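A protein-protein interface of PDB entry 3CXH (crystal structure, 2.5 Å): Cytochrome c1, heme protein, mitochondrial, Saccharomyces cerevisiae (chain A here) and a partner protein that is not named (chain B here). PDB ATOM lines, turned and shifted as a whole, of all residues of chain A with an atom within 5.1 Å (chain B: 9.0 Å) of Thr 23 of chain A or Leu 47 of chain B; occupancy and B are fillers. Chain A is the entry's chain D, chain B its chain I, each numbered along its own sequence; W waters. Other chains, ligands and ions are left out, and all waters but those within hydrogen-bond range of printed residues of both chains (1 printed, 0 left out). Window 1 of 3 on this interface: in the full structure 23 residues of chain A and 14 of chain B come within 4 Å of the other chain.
Printed residues of chain B within 4 Å of Ser 16 of chain A: Lys 46.
Of the printed residues of chain B, Phe 21 of chain A touches Trp 38 (3.96 Å), Tyr 39 (3.5 Å), His 42 (3.5 Å) and Asn 43 (2.9 Å).
Of chain B, only Tyr 39 (3.2 Å), Asn 43 (3.0 Å), Lys 46 (3.1 Å) and Leu 47 (3.8 Å) come within 4 Å of Thr 23 of chain A.
Printed residues of chain B within 4 Å of Asp 203 of chain A: Tyr 39 (3.1 Å).
Printed residues of chain A within 4 Å of Tyr 39 of chain B: Phe 21, Thr 23 and Asp 203.
Of the printed residues of chain A, Asn 43 of chain B touches Phe 21 (2.9 Å), Glu 22 (3.3 Å) and Thr 23 (3.0 Å).
Leu 47 of chain B touches just one residue of chain A: Thr 23.
The nearest residue of chain B that does not touch Thr 23 of chain A is His 42 of chain B (6.1 Å).
The nearest residue of chain A that does not touch Leu 47 of chain B is His 26 of chain A (4.1 Å).
The nearest printed residue of chain B that does not touch Phe 24 of chain A is Leu 47 of chain B (4.7 Å).
The side-chain amino group (NZ) of Lys 46 of chain B lies within hydrogen-bond range of the backbone carbonyl oxygen (O) of Ser 16 of chain A (3.0 Å).
O of Phe 21 of chain A is in hydrogen-bond range of ND2 of Asn 43 of chain B, at 2.9 Å.
The side-chain carboxylate of Glu 22 of chain A sits at hydrogen-bond distance from a ring nitrogen (NE2) of His 42 of chain B (2.6 Å).
The side-chain amide oxygen (OD1) of Asn 43 of chain B sits close to the side-chain carboxylate (OE2) of Glu 22 of chain A.
OE2 of Glu 22 of chain A lies within salt-bridge range of NZ of Lys 46 of chain B.
The backbone NH (N) of Thr 23 of chain A sits at hydrogen-bond distance from the side-chain amide oxygen (OD1) of Asn 43 of chain B (3.0 Å).
The backbone carbonyl oxygen (O) of Thr 23 of chain A sits close to the side-chain amino group (NZ) of Lys 46 of chain B (3.1 Å).
O of Lys 46 of chain B is in hydrogen-bond range of N of His 26 of chain A (2.7 Å).
O of Asp 203 of chain A is in hydrogen-bond range of OH of Tyr 39 of chain B, 3.1 Å away.
The backbone carbonyl oxygen of Phe 24 of chain A sits close to the backbone carbonyl oxygen of Lys 46 of chain B.
N of Phe 24 of chain A is in hydrogen-bond range of OD1 of Asp 203 of chain A (3.0 Å).
A ring nitrogen (NE2) of His 26 of chain A lies within hydrogen-bond range of the side-chain carboxylate of Asp 203 of chain A (2.7 Å).
The side-chain carboxylate (OD1) of Asp 203 of chain A sits at hydrogen-bond distance from a ring nitrogen (ND1) of His 202 of chain A (3.1 Å).
O of Tyr 39 of chain B sits at hydrogen-bond distance from ND2 of Asn 43 of chain B, 3.0 Å away.
NZ of Lys 46 of chain B lies within hydrogen-bond range of OD1 of Asn 43 of chain B, 2.7 Å away.
Among the printed residues, merely in contact across the chains: Thr 23 of chain A with Tyr 39 of chain B (3.2 Å), Phe 21 of chain A with Tyr 39 of chain B (3.5 Å), Phe 21 of chain A with His 42 of chain B (3.5 Å), Asp 25 of chain A with Lys 46 of chain B (3.7 Å), Thr 23 of chain A with Leu 47 of chain B (3.8 Å), His 26 of chain A with Trp 48 of chain B (3.9 Å) and Phe 21 of chain A with Trp 38 of chain B (3.96 Å).
Water W1 bridges the backbone NH of Trp 48 of chain B (3.1 Å) and a ring nitrogen (NE2) of His 26 of chain A (3.3 Å).
Of the 10 printed residues of chain A, 8 touch a printed residue of chain B.
Printed residues of chain A that touch a printed residue of chain B: Ser 16, Phe 21, Glu 22, Thr 23, Phe 24, Asp 25, His 26 and Asp 203.
Of the 19 printed residues of chain B, 7 touch a printed residue of chain A.
Among the printed residues, 17 pairs touch across the chains.
Among the printed residues, Asp or Glu carboxylates within 4 Å of a Lys or Arg side-chain nitrogen of the other chain: Glu 22 of chain A with Lys 46 of chain B (3.0 Å).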
ATOM      1  N   SER A  16     -22.344  29.194  -8.033  1.00  0.00           N
ATOM      2  CA  SER A  16     -21.142  28.765  -7.315  1.00  0.00           C
ATOM      3  C   SER A  16     -19.880  28.725  -8.178  1.00  0.00           C
ATOM      4  O   SER A  16     -18.770  28.554  -7.655  1.00  0.00           O
ATOM      5  CB  SER A  16     -21.365  27.418  -6.628  1.00  0.00           C
ATOM      6  OG  SER A  16     -21.782  26.444  -7.560  1.00  0.00           O
ATOM      7  N   HIS A  17     -20.056  28.826  -9.497  1.00  0.00           N
ATOM      8  CA  HIS A  17     -18.922  28.849 -10.418  1.00  0.00           C
ATOM      9  C   HIS A  17     -18.436  30.279 -10.652  1.00  0.00           C
ATOM     10  O   HIS A  17     -17.311  30.475 -11.094  1.00  0.00           O
ATOM     11  CB  HIS A  17     -19.208  28.118 -11.743  1.00  0.00           C
ATOM     12  CG  HIS A  17     -20.598  28.300 -12.270  1.00  0.00           C
ATOM     13  ND1 HIS A  17     -20.934  29.301 -13.156  1.00  0.00           N
ATOM     14  CD2 HIS A  17     -21.731  27.581 -12.070  1.00  0.00           C
ATOM     15  CE1 HIS A  17     -22.212  29.191 -13.482  1.00  0.00           C
ATOM     16  NE2 HIS A  17     -22.718  28.154 -12.837  1.00  0.00           N
ATOM     17  N   PHE A  21     -11.651  31.964  -8.349  1.00  0.00           N
ATOM     18  CA  PHE A  21     -11.154  30.726  -7.771  1.00  0.00           C
ATOM     19  C   PHE A  21     -12.149  29.578  -7.759  1.00  0.00           C
ATOM     20  O   PHE A  21     -11.814  28.479  -7.334  1.00  0.00           O
ATOM     21  CB  PHE A  21     -10.652  30.993  -6.354  1.00  0.00           C
ATOM     22  CG  PHE A  21      -9.829  32.251  -6.228  1.00  0.00           C
ATOM     23  CD1 PHE A  21     -10.202  33.255  -5.334  1.00  0.00           C
ATOM     24  CD2 PHE A  21      -8.694  32.441  -7.013  1.00  0.00           C
ATOM     25  CE1 PHE A  21      -9.456  34.434  -5.227  1.00  0.00           C
ATOM     26  CE2 PHE A  21      -7.941  33.610  -6.915  1.00  0.00           C
ATOM     27  CZ  PHE A  21      -8.322  34.613  -6.021  1.00  0.00           C
ATOM     28  N   GLU A  22     -13.338  29.798  -8.308  1.00  0.00           N
ATOM     29  CA  GLU A  22     -14.382  28.773  -8.276  1.00  0.00           C
ATOM     30  C   GLU A  22     -14.570  27.854  -9.472  1.00  0.00           C
ATOM     31  O   GLU A  22     -14.755  28.313 -10.600  1.00  0.00           O
ATOM     32  CB  GLU A  22     -15.742  29.417  -7.981  1.00  0.00           C
ATOM     33  CG  GLU A  22     -15.768  30.447  -6.854  1.00  0.00           C
ATOM     34  CD  GLU A  22     -15.187  29.935  -5.543  1.00  0.00           C
ATOM     35  OE1 GLU A  22     -14.517  30.737  -4.864  1.00  0.00           O
ATOM     36  OE2 GLU A  22     -15.397  28.752  -5.192  1.00  0.00           O
ATOM     37  N   THR A  23     -14.613  26.554  -9.199  1.00  0.00           N
ATOM     38  CA  THR A  23     -14.869  25.561 -10.235  1.00  0.00           C
ATOM     39  C   THR A  23     -16.381  25.397 -10.296  1.00  0.00           C
ATOM     40  O   THR A  23     -17.119  26.079  -9.593  1.00  0.00           O
ATOM     41  CB  THR A  23     -14.351  24.175  -9.850  1.00  0.00           C
ATOM     42  OG1 THR A  23     -15.019  23.737  -8.661  1.00  0.00           O
ATOM     43  CG2 THR A  23     -12.866  24.198  -9.630  1.00  0.00           C
ATOM     44  N   PHE A  24     -16.826  24.474 -11.131  1.00  0.00           N
ATOM     45  CA  PHE A  24     -18.237  24.159 -11.250  1.00  0.00           C
ATOM     46  C   PHE A  24     -18.581  23.237 -10.085  1.00  0.00           C
ATOM     47  O   PHE A  24     -17.694  22.616  -9.489  1.00  0.00           O
ATOM     48  CB  PHE A  24     -18.489  23.335 -12.512  1.00  0.00           C
ATOM     49  CG  PHE A  24     -18.573  24.132 -13.767  1.00  0.00           C
ATOM     50  CD1 PHE A  24     -17.903  23.702 -14.911  1.00  0.00           C
ATOM     51  CD2 PHE A  24     -19.378  25.264 -13.839  1.00  0.00           C
ATOM     52  CE1 PHE A  24     -18.041  24.387 -16.113  1.00  0.00           C
ATOM     53  CE2 PHE A  24     -19.521  25.955 -15.037  1.00  0.00           C
ATOM     54  CZ  PHE A  24     -18.850  25.511 -16.178  1.00  0.00           C
ATOM     55  N   ASP A  25     -19.872  23.150  -9.777  1.00  0.00           N
ATOM     56  CA  ASP A  25     -20.366  22.238  -8.749  1.00  0.00           C
ATOM     57  C   ASP A  25     -20.733  21.018  -9.588  1.00  0.00           C
ATOM     58  O   ASP A  25     -21.790  20.982 -10.237  1.00  0.00           O
ATOM     59  CB  ASP A  25     -21.613  22.810  -8.066  1.00  0.00           C
ATOM     60  CG  ASP A  25     -22.317  21.803  -7.157  1.00  0.00           C
ATOM     61  OD1 ASP A  25     -21.783  20.696  -6.907  1.00  0.00           O
ATOM     62  OD2 ASP A  25     -23.431  22.125  -6.692  1.00  0.00           O
ATOM     63  N   HIS A  26     -19.850  20.030  -9.597  1.00  0.00           N
ATOM     64  CA  HIS A  26     -20.084  18.844 -10.398  1.00  0.00           C
ATOM     65  C   HIS A  26     -21.314  18.009 -10.032  1.00  0.00           C
ATOM     66  O   HIS A  26     -21.783  17.200 -10.839  1.00  0.00           O
ATOM     67  CB  HIS A  26     -18.803  18.016 -10.496  1.00  0.00           C
ATOM     68  CG  HIS A  26     -17.737  18.679 -11.318  1.00  0.00           C
ATOM     69  ND1 HIS A  26     -17.292  18.165 -12.517  1.00  0.00           N
ATOM     70  CD2 HIS A  26     -17.064  19.841 -11.136  1.00  0.00           C
ATOM     71  CE1 HIS A  26     -16.395  18.982 -13.040  1.00  0.00           C
ATOM     72  NE2 HIS A  26     -16.239  20.005 -12.221  1.00  0.00           N
ATOM     73  N   HIS A 202     -13.572  25.264 -18.459  1.00  0.00           N
ATOM     74  CA  HIS A 202     -13.753  26.082 -17.254  1.00  0.00           C
ATOM     75  C   HIS A 202     -12.813  25.801 -16.073  1.00  0.00           C
ATOM     76  O   HIS A 202     -11.924  26.604 -15.786  1.00  0.00           O
ATOM     77  CB  HIS A 202     -15.215  25.995 -16.795  1.00  0.00           C
ATOM     78  CG  HIS A 202     -15.558  26.905 -15.655  1.00  0.00           C
ATOM     79  ND1 HIS A 202     -15.499  26.503 -14.336  1.00  0.00           N
ATOM     80  CD2 HIS A 202     -15.986  28.190 -15.639  1.00  0.00           C
ATOM     81  CE1 HIS A 202     -15.876  27.504 -13.558  1.00  0.00           C
ATOM     82  NE2 HIS A 202     -16.178  28.538 -14.323  1.00  0.00           N
ATOM     83  N   ASP A 203     -12.994  24.660 -15.413  1.00  0.00           N
ATOM     84  CA  ASP A 203     -12.174  24.313 -14.253  1.00  0.00           C
ATOM     85  C   ASP A 203     -10.678  24.433 -14.520  1.00  0.00           C
ATOM     86  O   ASP A 203      -9.956  25.132 -13.797  1.00  0.00           O
ATOM     87  CB  ASP A 203     -12.511  22.904 -13.737  1.00  0.00           C
ATOM     88  CG  ASP A 203     -13.908  22.807 -13.102  1.00  0.00           C
ATOM     89  OD1 ASP A 203     -14.679  23.800 -13.093  1.00  0.00           O
ATOM     90  OD2 ASP A 203     -14.237  21.710 -12.604  1.00  0.00           O
ATOM     91  N   THR B  36      -2.369  23.483  -7.353  1.00  0.00           N
ATOM     92  CA  THR B  36      -3.424  22.482  -7.501  1.00  0.00           C
ATOM     93  C   THR B  36      -4.072  22.124  -6.165  1.00  0.00           C
ATOM     94  O   THR B  36      -5.299  22.057  -6.058  1.00  0.00           O
ATOM     95  CB  THR B  36      -2.916  21.202  -8.181  1.00  0.00           C
ATOM     96  OG1 THR B  36      -2.329  21.525  -9.448  1.00  0.00           O
ATOM     97  CG2 THR B  36      -4.068  20.251  -8.412  1.00  0.00           C
ATOM     98  N   SER B  37      -3.250  21.918  -5.140  1.00  0.00           N
ATOM     99  CA  SER B  37      -3.758  21.577  -3.817  1.00  0.00           C
ATOM    100  C   SER B  37      -4.649  22.680  -3.269  1.00  0.00           C
ATOM    101  O   SER B  37      -5.754  22.411  -2.800  1.00  0.00           O
ATOM    102  CB  SER B  37      -2.607  21.307  -2.853  1.00  0.00           C
ATOM    103  OG  SER B  37      -1.937  20.120  -3.224  1.00  0.00           O
ATOM    104  N   TRP B  38      -4.177  23.922  -3.356  1.00  0.00           N
ATOM    105  CA  TRP B  38      -4.941  25.062  -2.867  1.00  0.00           C
ATOM    106  C   TRP B  38      -6.257  25.158  -3.630  1.00  0.00           C
ATOM    107  O   TRP B  38      -7.326  25.267  -3.032  1.00  0.00           O
ATOM    108  CB  TRP B  38      -4.150  26.359  -3.039  1.00  0.00           C
ATOM    109  CG  TRP B  38      -4.832  27.534  -2.406  1.00  0.00           C
ATOM    110  CD1 TRP B  38      -4.631  28.006  -1.143  1.00  0.00           C
ATOM    111  CD2 TRP B  38      -5.880  28.341  -2.973  1.00  0.00           C
ATOM    112  NE1 TRP B  38      -5.493  29.044  -0.879  1.00  0.00           N
ATOM    113  CE2 TRP B  38      -6.272  29.270  -1.983  1.00  0.00           C
ATOM    114  CE3 TRP B  38      -6.527  28.363  -4.216  1.00  0.00           C
ATOM    115  CZ2 TRP B  38      -7.285  30.216  -2.198  1.00  0.00           C
ATOM    116  CZ3 TRP B  38      -7.532  29.301  -4.431  1.00  0.00           C
ATOM    117  CH2 TRP B  38      -7.902  30.215  -3.424  1.00  0.00           C
ATOM    118  N   TYR B  39      -6.166  25.111  -4.955  1.00  0.00           N
ATOM    119  CA  TYR B  39      -7.333  25.196  -5.825  1.00  0.00           C
ATOM    120  C   TYR B  39      -8.352  24.097  -5.521  1.00  0.00           C
ATOM    121  O   TYR B  39      -9.540  24.378  -5.372  1.00  0.00           O
ATOM    122  CB  TYR B  39      -6.889  25.126  -7.292  1.00  0.00           C
ATOM    123  CG  TYR B  39      -7.977  25.420  -8.298  1.00  0.00           C
ATOM    124  CD1 TYR B  39      -8.471  26.715  -8.457  1.00  0.00           C
ATOM    125  CD2 TYR B  39      -8.494  24.411  -9.110  1.00  0.00           C
ATOM    126  CE1 TYR B  39      -9.452  27.003  -9.402  1.00  0.00           C
ATOM    127  CE2 TYR B  39      -9.474  24.687 -10.056  1.00  0.00           C
ATOM    128  CZ  TYR B  39      -9.946  25.987 -10.194  1.00  0.00           C
ATOM    129  OH  TYR B  39     -10.916  26.270 -11.123  1.00  0.00           O
ATOM    130  N   GLU B  40      -7.885  22.853  -5.431  1.00  0.00           N
ATOM    131  CA  GLU B  40      -8.772  21.721  -5.145  1.00  0.00           C
ATOM    132  C   GLU B  40      -9.380  21.789  -3.748  1.00  0.00           C
ATOM    133  O   GLU B  40     -10.549  21.451  -3.544  1.00  0.00           O
ATOM    134  CB  GLU B  40      -8.045  20.387  -5.322  1.00  0.00           C
ATOM    135  CG  GLU B  40      -7.921  19.945  -6.769  1.00  0.00           C
ATOM    136  CD  GLU B  40      -7.443  18.507  -6.912  1.00  0.00           C
ATOM    137  OE1 GLU B  40      -7.273  18.056  -8.066  1.00  0.00           O
ATOM    138  OE2 GLU B  40      -7.245  17.824  -5.880  1.00  0.00           O
ATOM    139  N   ASN B  41      -8.575  22.218  -2.788  1.00  0.00           N
ATOM    140  CA  ASN B  41      -9.043  22.334  -1.425  1.00  0.00           C
ATOM    141  C   ASN B  41     -10.094  23.435  -1.320  1.00  0.00           C
ATOM    142  O   ASN B  41     -11.058  23.310  -0.564  1.00  0.00           O
ATOM    143  CB  ASN B  41      -7.875  22.633  -0.492  1.00  0.00           C
ATOM    144  CG  ASN B  41      -8.338  23.038   0.882  1.00  0.00           C
ATOM    145  OD1 ASN B  41      -8.506  22.194   1.765  1.00  0.00           O
ATOM    146  ND2 ASN B  41      -8.603  24.332   1.062  1.00  0.00           N
ATOM    147  N   HIS B  42      -9.895  24.514  -2.073  1.00  0.00           N
ATOM    148  CA  HIS B  42     -10.811  25.653  -2.065  1.00  0.00           C
ATOM    149  C   HIS B  42     -12.177  25.264  -2.605  1.00  0.00           C
ATOM    150  O   HIS B  42     -13.191  25.856  -2.238  1.00  0.00           O
ATOM    151  CB  HIS B  42     -10.232  26.792  -2.907  1.00  0.00           C
ATOM    152  CG  HIS B  42     -11.123  27.990  -3.008  1.00  0.00           C
ATOM    153  ND1 HIS B  42     -11.037  29.056  -2.141  1.00  0.00           N
ATOM    154  CD2 HIS B  42     -12.116  28.292  -3.880  1.00  0.00           C
ATOM    155  CE1 HIS B  42     -11.940  29.964  -2.473  1.00  0.00           C
ATOM    156  NE2 HIS B  42     -12.607  29.524  -3.525  1.00  0.00           N
ATOM    157  N   ASN B  43     -12.192  24.266  -3.482  1.00  0.00           N
ATOM    158  CA  ASN B  43     -13.429  23.802  -4.092  1.00  0.00           C
ATOM    159  C   ASN B  43     -13.887  22.443  -3.590  1.00  0.00           C
ATOM    160  O   ASN B  43     -14.659  21.754  -4.263  1.00  0.00           O
ATOM    161  CB  ASN B  43     -13.286  23.802  -5.615  1.00  0.00           C
ATOM    162  CG  ASN B  43     -13.241  25.196  -6.180  1.00  0.00           C
ATOM    163  OD1 ASN B  43     -14.278  25.829  -6.340  1.00  0.00           O
ATOM    164  ND2 ASN B  43     -12.039  25.698  -6.447  1.00  0.00           N
ATOM    165  N   LYS B  44     -13.430  22.080  -2.394  1.00  0.00           N
ATOM    166  CA  LYS B  44     -13.792  20.808  -1.778  1.00  0.00           C
ATOM    167  C   LYS B  44     -15.312  20.655  -1.731  1.00  0.00           C
ATOM    168  O   LYS B  44     -16.029  21.519  -1.214  1.00  0.00           O
ATOM    169  CB  LYS B  44     -13.193  20.699  -0.371  1.00  0.00           C
ATOM    170  CG  LYS B  44     -13.639  19.455   0.403  1.00  0.00           C
ATOM    171  CD  LYS B  44     -12.850  19.271   1.706  1.00  0.00           C
ATOM    172  CE  LYS B  44     -11.459  18.677   1.455  1.00  0.00           C
ATOM    173  NZ  LYS B  44     -11.531  17.294   0.895  1.00  0.00           N
ATOM    174  N   GLY B  45     -15.793  19.574  -2.334  1.00  0.00           N
ATOM    175  CA  GLY B  45     -17.214  19.314  -2.373  1.00  0.00           C
ATOM    176  C   GLY B  45     -17.764  19.414  -3.778  1.00  0.00           C
ATOM    177  O   GLY B  45     -18.590  18.592  -4.178  1.00  0.00           O
ATOM    178  N   LYS B  46     -17.273  20.395  -4.535  1.00  0.00           N
ATOM    179  CA  LYS B  46     -17.720  20.641  -5.905  1.00  0.00           C
ATOM    180  C   LYS B  46     -17.091  19.747  -6.965  1.00  0.00           C
ATOM    181  O   LYS B  46     -17.710  19.477  -7.993  1.00  0.00           O
ATOM    182  CB  LYS B  46     -17.490  22.110  -6.266  1.00  0.00           C
ATOM    183  CG  LYS B  46     -18.506  23.064  -5.655  1.00  0.00           C
ATOM    184  CD  LYS B  46     -17.926  24.452  -5.424  1.00  0.00           C
ATOM    185  CE  LYS B  46     -17.489  25.106  -6.713  1.00  0.00           C
ATOM    186  NZ  LYS B  46     -16.937  26.465  -6.474  1.00  0.00           N
ATOM    187  N   LEU B  47     -15.874  19.278  -6.705  1.00  0.00           N
ATOM    188  CA  LEU B  47     -15.145  18.424  -7.645  1.00  0.00           C
ATOM    189  C   LEU B  47     -15.783  17.064  -7.863  1.00  0.00           C
ATOM    190  O   LEU B  47     -16.483  16.551  -6.993  1.00  0.00           O
ATOM    191  CB  LEU B  47     -13.707  18.218  -7.169  1.00  0.00           C
ATOM    192  CG  LEU B  47     -12.643  19.281  -7.430  1.00  0.00           C
ATOM    193  CD1 LEU B  47     -13.196  20.681  -7.264  1.00  0.00           C
ATOM    194  CD2 LEU B  47     -11.483  19.038  -6.477  1.00  0.00           C
ATOM    195  N   TRP B  48     -15.511  16.476  -9.024  1.00  0.00           N
ATOM    196  CA  TRP B  48     -16.037  15.162  -9.362  1.00  0.00           C
ATOM    197  C   TRP B  48     -15.574  14.123  -8.351  1.00  0.00           C
ATOM    198  O   TRP B  48     -16.371  13.300  -7.924  1.00  0.00           O
ATOM    199  CB  TRP B  48     -15.592  14.742 -10.760  1.00  0.00           C
ATOM    200  CG  TRP B  48     -15.910  13.314 -11.074  1.00  0.00           C
ATOM    201  CD1 TRP B  48     -15.026  12.330 -11.416  1.00  0.00           C
ATOM    202  CD2 TRP B  48     -17.206  12.704 -11.069  1.00  0.00           C
ATOM    203  NE1 TRP B  48     -15.691  11.148 -11.629  1.00  0.00           N
ATOM    204  CE2 TRP B  48     -17.031  11.348 -11.424  1.00  0.00           C
ATOM    205  CE3 TRP B  48     -18.502  13.171 -10.793  1.00  0.00           C
ATOM    206  CZ2 TRP B  48     -18.098  10.453 -11.513  1.00  0.00           C
ATOM    207  CZ3 TRP B  48     -19.565  12.279 -10.879  1.00  0.00           C
ATOM    208  CH2 TRP B  48     -19.355  10.935 -11.237  1.00  0.00           C
ATOM    209  N   LYS B  49     -14.290  14.153  -7.997  1.00  0.00           N
ATOM    210  CA  LYS B  49     -13.726  13.213  -7.026  1.00  0.00           C
ATOM    211  C   LYS B  49     -14.586  13.207  -5.778  1.00  0.00           C
ATOM    212  O   LYS B  49     -14.995  12.155  -5.290  1.00  0.00           O
ATOM    213  CB  LYS B  49     -12.322  13.629  -6.592  1.00  0.00           C
ATOM    214  CG  LYS B  49     -11.271  13.661  -7.670  1.00  0.00           C
ATOM    215  CD  LYS B  49      -9.886  13.769  -7.038  1.00  0.00           C
ATOM    216  CE  LYS B  49      -9.806  14.913  -6.029  1.00  0.00           C
ATOM    217  NZ  LYS B  49      -8.469  14.960  -5.369  1.00  0.00           N
ATOM    218  N   ASP B  50     -14.844  14.408  -5.271  1.00  0.00           N
ATOM    219  CA  ASP B  50     -15.642  14.596  -4.074  1.00  0.00           C
ATOM    220  C   ASP B  50     -17.049  14.026  -4.245  1.00  0.00           C
ATOM    221  O   ASP B  50     -17.527  13.289  -3.387  1.00  0.00           O
ATOM    222  CB  ASP B  50     -15.678  16.086  -3.704  1.00  0.00           C
ATOM    223  CG  ASP B  50     -14.275  16.688  -3.538  1.00  0.00           C
ATOM    224  OD1 ASP B  50     -14.109  17.895  -3.806  1.00  0.00           O
ATOM    225  OD2 ASP B  50     -13.336  15.963  -3.141  1.00  0.00           O
ATOM    226  N   VAL B  51     -17.678  14.310  -5.380  1.00  0.00           N
ATOM    227  CA  VAL B  51     -19.025  13.822  -5.669  1.00  0.00           C
ATOM    228  C   VAL B  51     -19.057  12.311  -5.948  1.00  0.00           C
ATOM    229  O   VAL B  51     -20.052  11.642  -5.670  1.00  0.00           O
ATOM    230  CB  VAL B  51     -19.633  14.593  -6.862  1.00  0.00           C
ATOM    231  CG1 VAL B  51     -21.019  14.068  -7.205  1.00  0.00           C
ATOM    232  CG2 VAL B  51     -19.698  16.078  -6.539  1.00  0.00           C
ATOM    233  N   LYS B  52     -17.953  11.777  -6.463  1.00  0.00           N
ATOM    234  CA  LYS B  52     -17.839  10.353  -6.786  1.00  0.00           C
ATOM    235  C   LYS B  52     -17.747   9.460  -5.547  1.00  0.00           C
ATOM    236  O   LYS B  52     -18.242   8.331  -5.554  1.00  0.00           O
ATOM    237  CB  LYS B  52     -16.619  10.115  -7.675  1.00  0.00           C
ATOM    238  CG  LYS B  52     -16.464   8.691  -8.173  1.00  0.00           C
ATOM    239  CD  LYS B  52     -15.086   8.491  -8.774  1.00  0.00           C
ATOM    240  CE  LYS B  52     -14.884   7.064  -9.242  1.00  0.00           C
ATOM    241  NZ  LYS B  52     -13.466   6.829  -9.609  1.00  0.00           N
ATOM    242  N   ALA B  53     -17.074   9.952  -4.507  1.00  0.00           N
ATOM    243  CA  ALA B  53     -16.910   9.209  -3.254  1.00  0.00           C
ATOM    244  C   ALA B  53     -18.262   9.062  -2.557  1.00  0.00           C
ATOM    245  O   ALA B  53     -18.704   7.949  -2.263  1.00  0.00           O
ATOM    246  CB  ALA B  53     -15.914   9.923  -2.340  1.00  0.00           C
ATOM    247  N   ARG B  54     -18.912  10.200  -2.315  1.00  0.00           N
ATOM    248  CA  ARG B  54     -20.226  10.244  -1.678  1.00  0.00           C
ATOM    249  C   ARG B  54     -21.182   9.384  -2.503  1.00  0.00           C
ATOM    250  O   ARG B  54     -21.419   8.218  -2.180  1.00  0.00           O
ATOM    251  CB  ARG B  54     -20.723  11.695  -1.623  1.00  0.00           C
ATOM    252  CG  ARG B  54     -19.885  12.612  -0.730  1.00  0.00           C
ATOM    253  CD  ARG B  54     -19.945  14.079  -1.170  1.00  0.00           C
ATOM    254  NE  ARG B  54     -21.304  14.619  -1.219  1.00  0.00           N
ATOM    255  CZ  ARG B  54     -21.641  15.754  -1.829  1.00  0.00           C
ATOM    256  NH1 ARG B  54     -20.719  16.483  -2.448  1.00  0.00           N
ATOM    257  NH2 ARG B  54     -22.905  16.159  -1.830  1.00  0.00           N
HETATM  258  O   HOH W   1     -13.796  18.081 -10.996  1.00  0.00           O
